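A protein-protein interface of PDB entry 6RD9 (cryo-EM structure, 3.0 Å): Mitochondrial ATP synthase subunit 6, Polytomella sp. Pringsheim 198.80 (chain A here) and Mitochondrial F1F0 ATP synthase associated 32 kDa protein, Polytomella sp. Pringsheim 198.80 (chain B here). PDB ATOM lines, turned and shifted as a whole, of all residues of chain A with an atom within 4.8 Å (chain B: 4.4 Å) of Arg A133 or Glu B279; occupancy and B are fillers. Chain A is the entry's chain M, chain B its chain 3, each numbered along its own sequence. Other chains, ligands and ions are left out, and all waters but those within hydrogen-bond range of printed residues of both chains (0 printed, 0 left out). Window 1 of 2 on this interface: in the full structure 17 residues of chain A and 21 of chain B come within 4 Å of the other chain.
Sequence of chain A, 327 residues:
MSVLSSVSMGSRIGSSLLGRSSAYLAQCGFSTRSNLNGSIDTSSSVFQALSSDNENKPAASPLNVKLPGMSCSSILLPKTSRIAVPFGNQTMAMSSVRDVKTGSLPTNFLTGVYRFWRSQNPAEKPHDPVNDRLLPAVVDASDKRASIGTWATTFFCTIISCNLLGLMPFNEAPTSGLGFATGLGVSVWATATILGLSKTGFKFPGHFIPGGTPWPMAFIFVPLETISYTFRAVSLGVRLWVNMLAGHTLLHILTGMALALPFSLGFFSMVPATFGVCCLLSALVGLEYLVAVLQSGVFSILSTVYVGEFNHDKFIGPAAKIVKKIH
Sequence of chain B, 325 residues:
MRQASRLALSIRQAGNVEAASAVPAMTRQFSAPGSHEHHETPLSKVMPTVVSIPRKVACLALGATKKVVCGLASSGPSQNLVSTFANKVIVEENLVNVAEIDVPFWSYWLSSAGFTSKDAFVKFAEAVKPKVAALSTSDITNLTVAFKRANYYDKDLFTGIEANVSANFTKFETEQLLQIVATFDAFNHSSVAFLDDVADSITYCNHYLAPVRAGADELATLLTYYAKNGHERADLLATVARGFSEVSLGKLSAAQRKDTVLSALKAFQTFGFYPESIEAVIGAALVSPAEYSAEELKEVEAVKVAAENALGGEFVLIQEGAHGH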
ATOM      1  N   ASN A 131     -11.730  17.805 -11.418  1.00  0.00           N
ATOM      2  CA  ASN A 131     -10.843  17.299 -10.386  1.00  0.00           C
ATOM      3  C   ASN A 131     -11.463  15.995  -9.911  1.00  0.00           C
ATOM      4  O   ASN A 131     -12.348  15.453 -10.574  1.00  0.00           O
ATOM      5  CB  ASN A 131     -10.641  18.358  -9.301  1.00  0.00           C
ATOM      6  CG  ASN A 131     -11.932  18.995  -8.854  1.00  0.00           C
ATOM      7  OD1 ASN A 131     -13.017  18.544  -9.189  1.00  0.00           O
ATOM      8  ND2 ASN A 131     -11.816  20.082  -8.116  1.00  0.00           N
ATOM      9  N   ASP A 132     -11.028  15.478  -8.762  1.00  0.00           N
ATOM     10  CA  ASP A 132     -11.567  14.211  -8.269  1.00  0.00           C
ATOM     11  C   ASP A 132     -13.021  14.301  -7.845  1.00  0.00           C
ATOM     12  O   ASP A 132     -13.653  13.265  -7.641  1.00  0.00           O
ATOM     13  CB  ASP A 132     -10.768  13.696  -7.083  1.00  0.00           C
ATOM     14  CG  ASP A 132      -9.398  13.222  -7.459  1.00  0.00           C
ATOM     15  OD1 ASP A 132      -8.446  14.018  -7.349  1.00  0.00           O
ATOM     16  OD2 ASP A 132      -9.265  12.044  -7.843  1.00  0.00           O
ATOM     17  N   ARG A 133     -13.551  15.500  -7.665  1.00  0.00           N
ATOM     18  CA  ARG A 133     -14.975  15.650  -7.435  1.00  0.00           C
ATOM     19  C   ARG A 133     -15.750  15.398  -8.715  1.00  0.00           C
ATOM     20  O   ARG A 133     -16.755  14.685  -8.710  1.00  0.00           O
ATOM     21  CB  ARG A 133     -15.256  17.049  -6.903  1.00  0.00           C
ATOM     22  CG  ARG A 133     -16.701  17.338  -6.620  1.00  0.00           C
ATOM     23  CD  ARG A 133     -17.143  16.767  -5.307  1.00  0.00           C
ATOM     24  NE  ARG A 133     -18.576  16.929  -5.153  1.00  0.00           N
ATOM     25  CZ  ARG A 133     -19.452  15.989  -5.458  1.00  0.00           C
ATOM     26  NH1 ARG A 133     -19.025  14.829  -5.909  1.00  0.00           N
ATOM     27  NH2 ARG A 133     -20.742  16.199  -5.307  1.00  0.00           N
ATOM     28  N   LEU A 134     -15.273  15.941  -9.820  1.00  0.00           N
ATOM     29  CA  LEU A 134     -15.981  15.889 -11.082  1.00  0.00           C
ATOM     30  C   LEU A 134     -15.613  14.676 -11.915  1.00  0.00           C
ATOM     31  O   LEU A 134     -16.176  14.486 -12.989  1.00  0.00           O
ATOM     32  CB  LEU A 134     -15.690  17.160 -11.863  1.00  0.00           C
ATOM     33  CG  LEU A 134     -16.768  17.651 -12.802  1.00  0.00           C
ATOM     34  CD1 LEU A 134     -17.928  18.059 -11.986  1.00  0.00           C
ATOM     35  CD2 LEU A 134     -16.272  18.791 -13.615  1.00  0.00           C
ATOM     36  N   LEU A 135     -14.692  13.846 -11.450  1.00  0.00           N
ATOM     37  CA  LEU A 135     -14.241  12.724 -12.262  1.00  0.00           C
ATOM     38  C   LEU A 135     -15.272  11.624 -12.453  1.00  0.00           C
ATOM     39  O   LEU A 135     -15.287  11.045 -13.548  1.00  0.00           O
ATOM     40  CB  LEU A 135     -12.950  12.132 -11.698  1.00  0.00           C
ATOM     41  CG  LEU A 135     -11.634  12.624 -12.261  1.00  0.00           C
ATOM     42  CD1 LEU A 135     -10.566  11.759 -11.694  1.00  0.00           C
ATOM     43  CD2 LEU A 135     -11.635  12.592 -13.756  1.00  0.00           C
ATOM     44  N   PRO A 136     -16.125  11.253 -11.490  1.00  0.00           N
ATOM     45  CA  PRO A 136     -17.206  10.335 -11.852  1.00  0.00           C
ATOM     46  C   PRO A 136     -18.260  10.944 -12.726  1.00  0.00           C
ATOM     47  O   PRO A 136     -18.964  10.200 -13.404  1.00  0.00           O
ATOM     48  CB  PRO A 136     -17.786   9.930 -10.504  1.00  0.00           C
ATOM     49  CG  PRO A 136     -16.735  10.073  -9.630  1.00  0.00           C
ATOM     50  CD  PRO A 136     -15.986  11.258 -10.027  1.00  0.00           C
ATOM     51  N   PRO A 318     -21.909  17.889  -9.358  1.00  0.00           N
ATOM     52  CA  PRO A 318     -22.067  17.962  -7.904  1.00  0.00           C
ATOM     53  C   PRO A 318     -23.414  18.550  -7.515  1.00  0.00           C
ATOM     54  O   PRO A 318     -23.778  19.646  -7.943  1.00  0.00           O
ATOM     55  CB  PRO A 318     -20.917  18.871  -7.466  1.00  0.00           C
ATOM     56  CG  PRO A 318     -20.561  19.637  -8.669  1.00  0.00           C
ATOM     57  CD  PRO A 318     -20.844  18.775  -9.839  1.00  0.00           C
ATOM     58  N   ALA A 319     -24.154  17.808  -6.699  1.00  0.00           N
ATOM     59  CA  ALA A 319     -25.397  18.302  -6.135  1.00  0.00           C
ATOM     60  C   ALA A 319     -25.205  19.004  -4.802  1.00  0.00           C
ATOM     61  O   ALA A 319     -26.132  19.658  -4.324  1.00  0.00           O
ATOM     62  CB  ALA A 319     -26.387  17.156  -5.950  1.00  0.00           C
ATOM     63  N   ALA A 320     -24.033  18.887  -4.192  1.00  0.00           N
ATOM     64  CA  ALA A 320     -23.744  19.555  -2.940  1.00  0.00           C
ATOM     65  C   ALA A 320     -22.279  19.942  -2.910  1.00  0.00           C
ATOM     66  O   ALA A 320     -21.418  19.186  -3.350  1.00  0.00           O
ATOM     67  CB  ALA A 320     -24.082  18.668  -1.756  1.00  0.00           C
ATOM     68  N   LYS A 321     -21.998  21.118  -2.373  1.00  0.00           N
ATOM     69  CA  LYS A 321     -20.671  21.694  -2.464  1.00  0.00           C
ATOM     70  C   LYS A 321     -20.259  22.233  -1.105  1.00  0.00           C
ATOM     71  O   LYS A 321     -21.087  22.423  -0.218  1.00  0.00           O
ATOM     72  CB  LYS A 321     -20.632  22.805  -3.514  1.00  0.00           C
ATOM     73  CG  LYS A 321     -19.306  22.959  -4.208  1.00  0.00           C
ATOM     74  CD  LYS A 321     -19.182  24.302  -4.882  1.00  0.00           C
ATOM     75  CE  LYS A 321     -20.131  24.424  -6.048  1.00  0.00           C
ATOM     76  NZ  LYS A 321     -19.948  25.720  -6.748  1.00  0.00           N
ATOM     77  N   ILE A 322     -18.960  22.436  -0.937  1.00  0.00           N
ATOM     78  CA  ILE A 322     -18.399  23.165   0.192  1.00  0.00           C
ATOM     79  C   ILE A 322     -17.598  24.307  -0.418  1.00  0.00           C
ATOM     80  O   ILE A 322     -16.450  24.133  -0.842  1.00  0.00           O
ATOM     81  CB  ILE A 322     -17.555  22.264   1.100  1.00  0.00           C
ATOM     82  CG1 ILE A 322     -18.469  21.235   1.751  1.00  0.00           C
ATOM     83  CG2 ILE A 322     -16.836  23.044   2.166  1.00  0.00           C
ATOM     84  CD1 ILE A 322     -17.805  20.337   2.710  1.00  0.00           C
ATOM     85  N   SER B 245     -19.978   9.589  -5.560  1.00  0.00           N
ATOM     86  CA  SER B 245     -20.484  10.762  -6.234  1.00  0.00           C
ATOM     87  C   SER B 245     -21.995  10.658  -6.281  1.00  0.00           C
ATOM     88  O   SER B 245     -22.586   9.728  -5.730  1.00  0.00           O
ATOM     89  CB  SER B 245     -19.881  10.895  -7.632  1.00  0.00           C
ATOM     90  OG  SER B 245     -20.373  12.050  -8.279  1.00  0.00           O
ATOM     91  N   GLU B 246     -22.625  11.627  -6.934  1.00  0.00           N
ATOM     92  CA  GLU B 246     -24.051  11.536  -7.193  1.00  0.00           C
ATOM     93  C   GLU B 246     -24.364  10.397  -8.138  1.00  0.00           C
ATOM     94  O   GLU B 246     -25.444   9.805  -8.060  1.00  0.00           O
ATOM     95  CB  GLU B 246     -24.550  12.842  -7.786  1.00  0.00           C
ATOM     96  CG  GLU B 246     -24.623  13.968  -6.803  1.00  0.00           C
ATOM     97  CD  GLU B 246     -23.316  14.700  -6.653  1.00  0.00           C
ATOM     98  OE1 GLU B 246     -22.345  14.332  -7.338  1.00  0.00           O
ATOM     99  OE2 GLU B 246     -23.255  15.642  -5.841  1.00  0.00           O
ATOM    100  N   GLU B 276     -12.525  16.098  -0.873  1.00  0.00           N
ATOM    101  CA  GLU B 276     -13.473  17.004  -1.502  1.00  0.00           C
ATOM    102  C   GLU B 276     -14.691  16.284  -2.034  1.00  0.00           C
ATOM    103  O   GLU B 276     -15.674  16.935  -2.366  1.00  0.00           O
ATOM    104  CB  GLU B 276     -12.816  17.776  -2.638  1.00  0.00           C
ATOM    105  CG  GLU B 276     -13.387  19.164  -2.854  1.00  0.00           C
ATOM    106  CD  GLU B 276     -13.043  19.723  -4.209  1.00  0.00           C
ATOM    107  OE1 GLU B 276     -12.390  19.007  -4.991  1.00  0.00           O
ATOM    108  OE2 GLU B 276     -13.427  20.872  -4.501  1.00  0.00           O
ATOM    109  N   SER B 277     -14.646  14.965  -2.146  1.00  0.00           N
ATOM    110  CA  SER B 277     -15.801  14.187  -2.545  1.00  0.00           C
ATOM    111  C   SER B 277     -16.500  13.568  -1.362  1.00  0.00           C
ATOM    112  O   SER B 277     -17.170  12.548  -1.516  1.00  0.00           O
ATOM    113  CB  SER B 277     -15.397  13.099  -3.524  1.00  0.00           C
ATOM    114  OG  SER B 277     -14.802  12.030  -2.830  1.00  0.00           O
ATOM    115  N   ILE B 278     -16.315  14.130  -0.165  1.00  0.00           N
ATOM    116  CA  ILE B 278     -17.201  13.787   0.940  1.00  0.00           C
ATOM    117  C   ILE B 278     -18.477  14.596   0.855  1.00  0.00           C
ATOM    118  O   ILE B 278     -19.494  14.208   1.428  1.00  0.00           O
ATOM    119  CB  ILE B 278     -16.515  13.972   2.308  1.00  0.00           C
ATOM    120  CG1 ILE B 278     -17.154  13.064   3.348  1.00  0.00           C
ATOM    121  CG2 ILE B 278     -16.576  15.398   2.783  1.00  0.00           C
ATOM    122  CD1 ILE B 278     -16.421  13.033   4.631  1.00  0.00           C
ATOM    123  N   GLU B 279     -18.484  15.660   0.071  1.00  0.00           N
ATOM    124  CA  GLU B 279     -19.676  16.464  -0.082  1.00  0.00           C
ATOM    125  C   GLU B 279     -20.684  15.851  -1.038  1.00  0.00           C
ATOM    126  O   GLU B 279     -21.674  16.499  -1.364  1.00  0.00           O
ATOM    127  CB  GLU B 279     -19.277  17.857  -0.532  1.00  0.00           C
ATOM    128  CG  GLU B 279     -18.722  17.916  -1.897  1.00  0.00           C
ATOM    129  CD  GLU B 279     -17.847  19.117  -2.091  1.00  0.00           C
ATOM    130  OE1 GLU B 279     -17.509  19.755  -1.088  1.00  0.00           O
ATOM    131  OE2 GLU B 279     -17.497  19.438  -3.239  1.00  0.00           O
ATOM    132  N   ALA B 280     -20.453  14.636  -1.510  1.00  0.00           N
ATOM    133  CA  ALA B 280     -21.435  13.884  -2.267  1.00  0.00           C
ATOM    134  C   ALA B 280     -22.047  12.755  -1.474  1.00  0.00           C
ATOM    135  O   ALA B 280     -23.088  12.232  -1.877  1.00  0.00           O
ATOM    136  CB  ALA B 280     -20.799  13.296  -3.515  1.00  0.00           C
ATOM    137  N   VAL B 281     -21.410  12.340  -0.386  1.00  0.00           N
ATOM    138  CA  VAL B 281     -21.958  11.290   0.454  1.00  0.00           C
ATOM    139  C   VAL B 281     -22.691  11.977   1.599  1.00  0.00           C
ATOM    140  O   VAL B 281     -23.686  11.458   2.108  1.00  0.00           O
ATOM    141  CB  VAL B 281     -20.856  10.306   0.909  1.00  0.00           C
ATOM    142  CG1 VAL B 281     -19.739  10.999   1.593  1.00  0.00           C
ATOM    143  CG2 VAL B 281     -21.390   9.210   1.776  1.00  0.00           C
ATOM    144  N   ILE B 282     -22.256  13.183   1.965  1.00  0.00           N
ATOM    145  CA  ILE B 282     -23.048  13.990   2.887  1.00  0.00           C
ATOM    146  C   ILE B 282     -24.304  14.491   2.196  1.00  0.00           C
ATOM    147  O   ILE B 282     -25.417  14.312   2.696  1.00  0.00           O
ATOM    148  CB  ILE B 282     -22.223  15.159   3.446  1.00  0.00           C
ATOM    149  CG1 ILE B 282     -21.087  14.656   4.312  1.00  0.00           C
ATOM    150  CG2 ILE B 282     -23.082  16.018   4.293  1.00  0.00           C
ATOM    151  CD1 ILE B 282     -20.136  15.744   4.679  1.00  0.00           C
ATOM    152  N   GLY B 283     -24.155  15.064   1.004  1.00  0.00           N
ATOM    153  CA  GLY B 283     -25.283  15.563   0.244  1.00  0.00           C
ATOM    154  C   GLY B 283     -26.222  14.494  -0.270  1.00  0.00           C
ATOM    155  O   GLY B 283     -27.277  14.829  -0.807  1.00  0.00           O
ATOM    156  N   PHE B 315     -21.023  24.013   3.888  1.00  0.00           N
ATOM    157  CA  PHE B 315     -21.821  23.132   3.055  1.00  0.00           C
ATOM    158  C   PHE B 315     -23.011  23.870   2.472  1.00  0.00           C
ATOM    159  O   PHE B 315     -23.641  24.687   3.144  1.00  0.00           O
ATOM    160  CB  PHE B 315     -22.313  21.969   3.893  1.00  0.00           C
ATOM    161  CG  PHE B 315     -22.611  20.753   3.119  1.00  0.00           C
ATOM    162  CD1 PHE B 315     -21.625  19.818   2.889  1.00  0.00           C
ATOM    163  CD2 PHE B 315     -23.880  20.521   2.643  1.00  0.00           C
ATOM    164  CE1 PHE B 315     -21.894  18.687   2.186  1.00  0.00           C
ATOM    165  CE2 PHE B 315     -24.153  19.390   1.943  1.00  0.00           C
ATOM    166  CZ  PHE B 315     -23.164  18.474   1.710  1.00  0.00           C
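Printed residues of chain B within 4 Å of Asn A131: Glu B276. Of the printed residues of chain B, Arg A133 touches Ser B245 (3.9 Å), Glu B246 (2.6 Å), Glu B276 (3.3 Å), Glu B279 (3.3 Å) and Ala B280 (3.4 Å). Leu A135 touches none of the printed residues of chain B. Of the printed residues of chain B, Ile A322 touches Glu B279 (3.1 Å) and Phe B315 (3.6 Å). Of the printed residues of chain A, Ser B245 touches Arg A133 (3.9 Å) and Pro A136 (3.7 Å). Glu B279 touches just these residues of chain A: Arg A133 (3.3 Å), Ala A320 (3.3 Å), Lys A321 (3.7 Å) and Ile A322 (3.1 Å). Printed residues of chain A within 4 Å of Gly B283: Ala A320 (3.9 Å). The nearest printed residue of chain B that does not touch Arg A133 is Ser B277 (4.01 Å). The nearest printed residue of chain A that does not touch Glu B279 is Pro A318 (5.5 Å). The nearest printed residue of chain B that does not touch Ala A320 is Ala B280 (5.0 Å).
The side-chain amide nitrogen (ND2) of Asn A131 sits at hydrogen-bond distance from the side-chain carboxylate (OE1) of Glu B276 (3.4 Å). OE2 of Glu B246 is in salt-bridge range of NH2 of Arg A133 (2.6 Å). The guanidinium group of Arg A133 is in salt-bridge range of the side-chain carboxylate of Glu B279 (3.3 Å). The backbone NH of Ala A319 is in hydrogen-bond range of the side-chain carboxylate of Glu B246, 2.5 Å away. The side-chain carboxylate (OE1) of Glu B279 is in hydrogen-bond range of the backbone NH (N) of Ile A322 (3.1 Å). O of Ala A320 lies close to O of Glu B279.
The backbone NH (N) of Arg A133 sits close to the side-chain amide oxygen (OD1) of Asn A131 (3.4 Å). The side-chain hydroxyl (OG) of Ser B245 lies within hydrogen-bond range of the side-chain carboxylate (OE1) of Glu B246.
Hydrophobic or aromatic side chains of chain A that line the printed part of chain B: Pro A136, Ala A319, Ala A320 and Ile A322. Along chain A the printed residues that touch a printed residue of chain B span positions 131 to 322. Of the 11 printed residues of chain B, 7 touch a printed residue of chain A. Among the printed residues, Asp or Glu carboxylates within 4 Å of a Lys or Arg side-chain nitrogen of the other chain: Arg A133 with Glu B246 and Arg A133 with Glu B279.
Among the printed residues, pairs that only touch across the chains: Arg A133 with Ser B245 (3.9 Å), Arg A133 with Glu B276 (3.3 Å), Arg A133 with Ala B280 (3.4 Å), Pro A136 with Ser B245 (3.7 Å), Pro A318 with Glu B246 (3.3 Å), Ala A320 with Glu B246 (3.7 Å), Ala A320 with Gly B283 (3.9 Å), Ala A320 with Phe B315 (3.6 Å), Lys A321 with Glu B279 (3.7 Å), Lys A321 with Phe B315 (3.4 Å) and Ile A322 with Phe B315 (3.6 Å).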
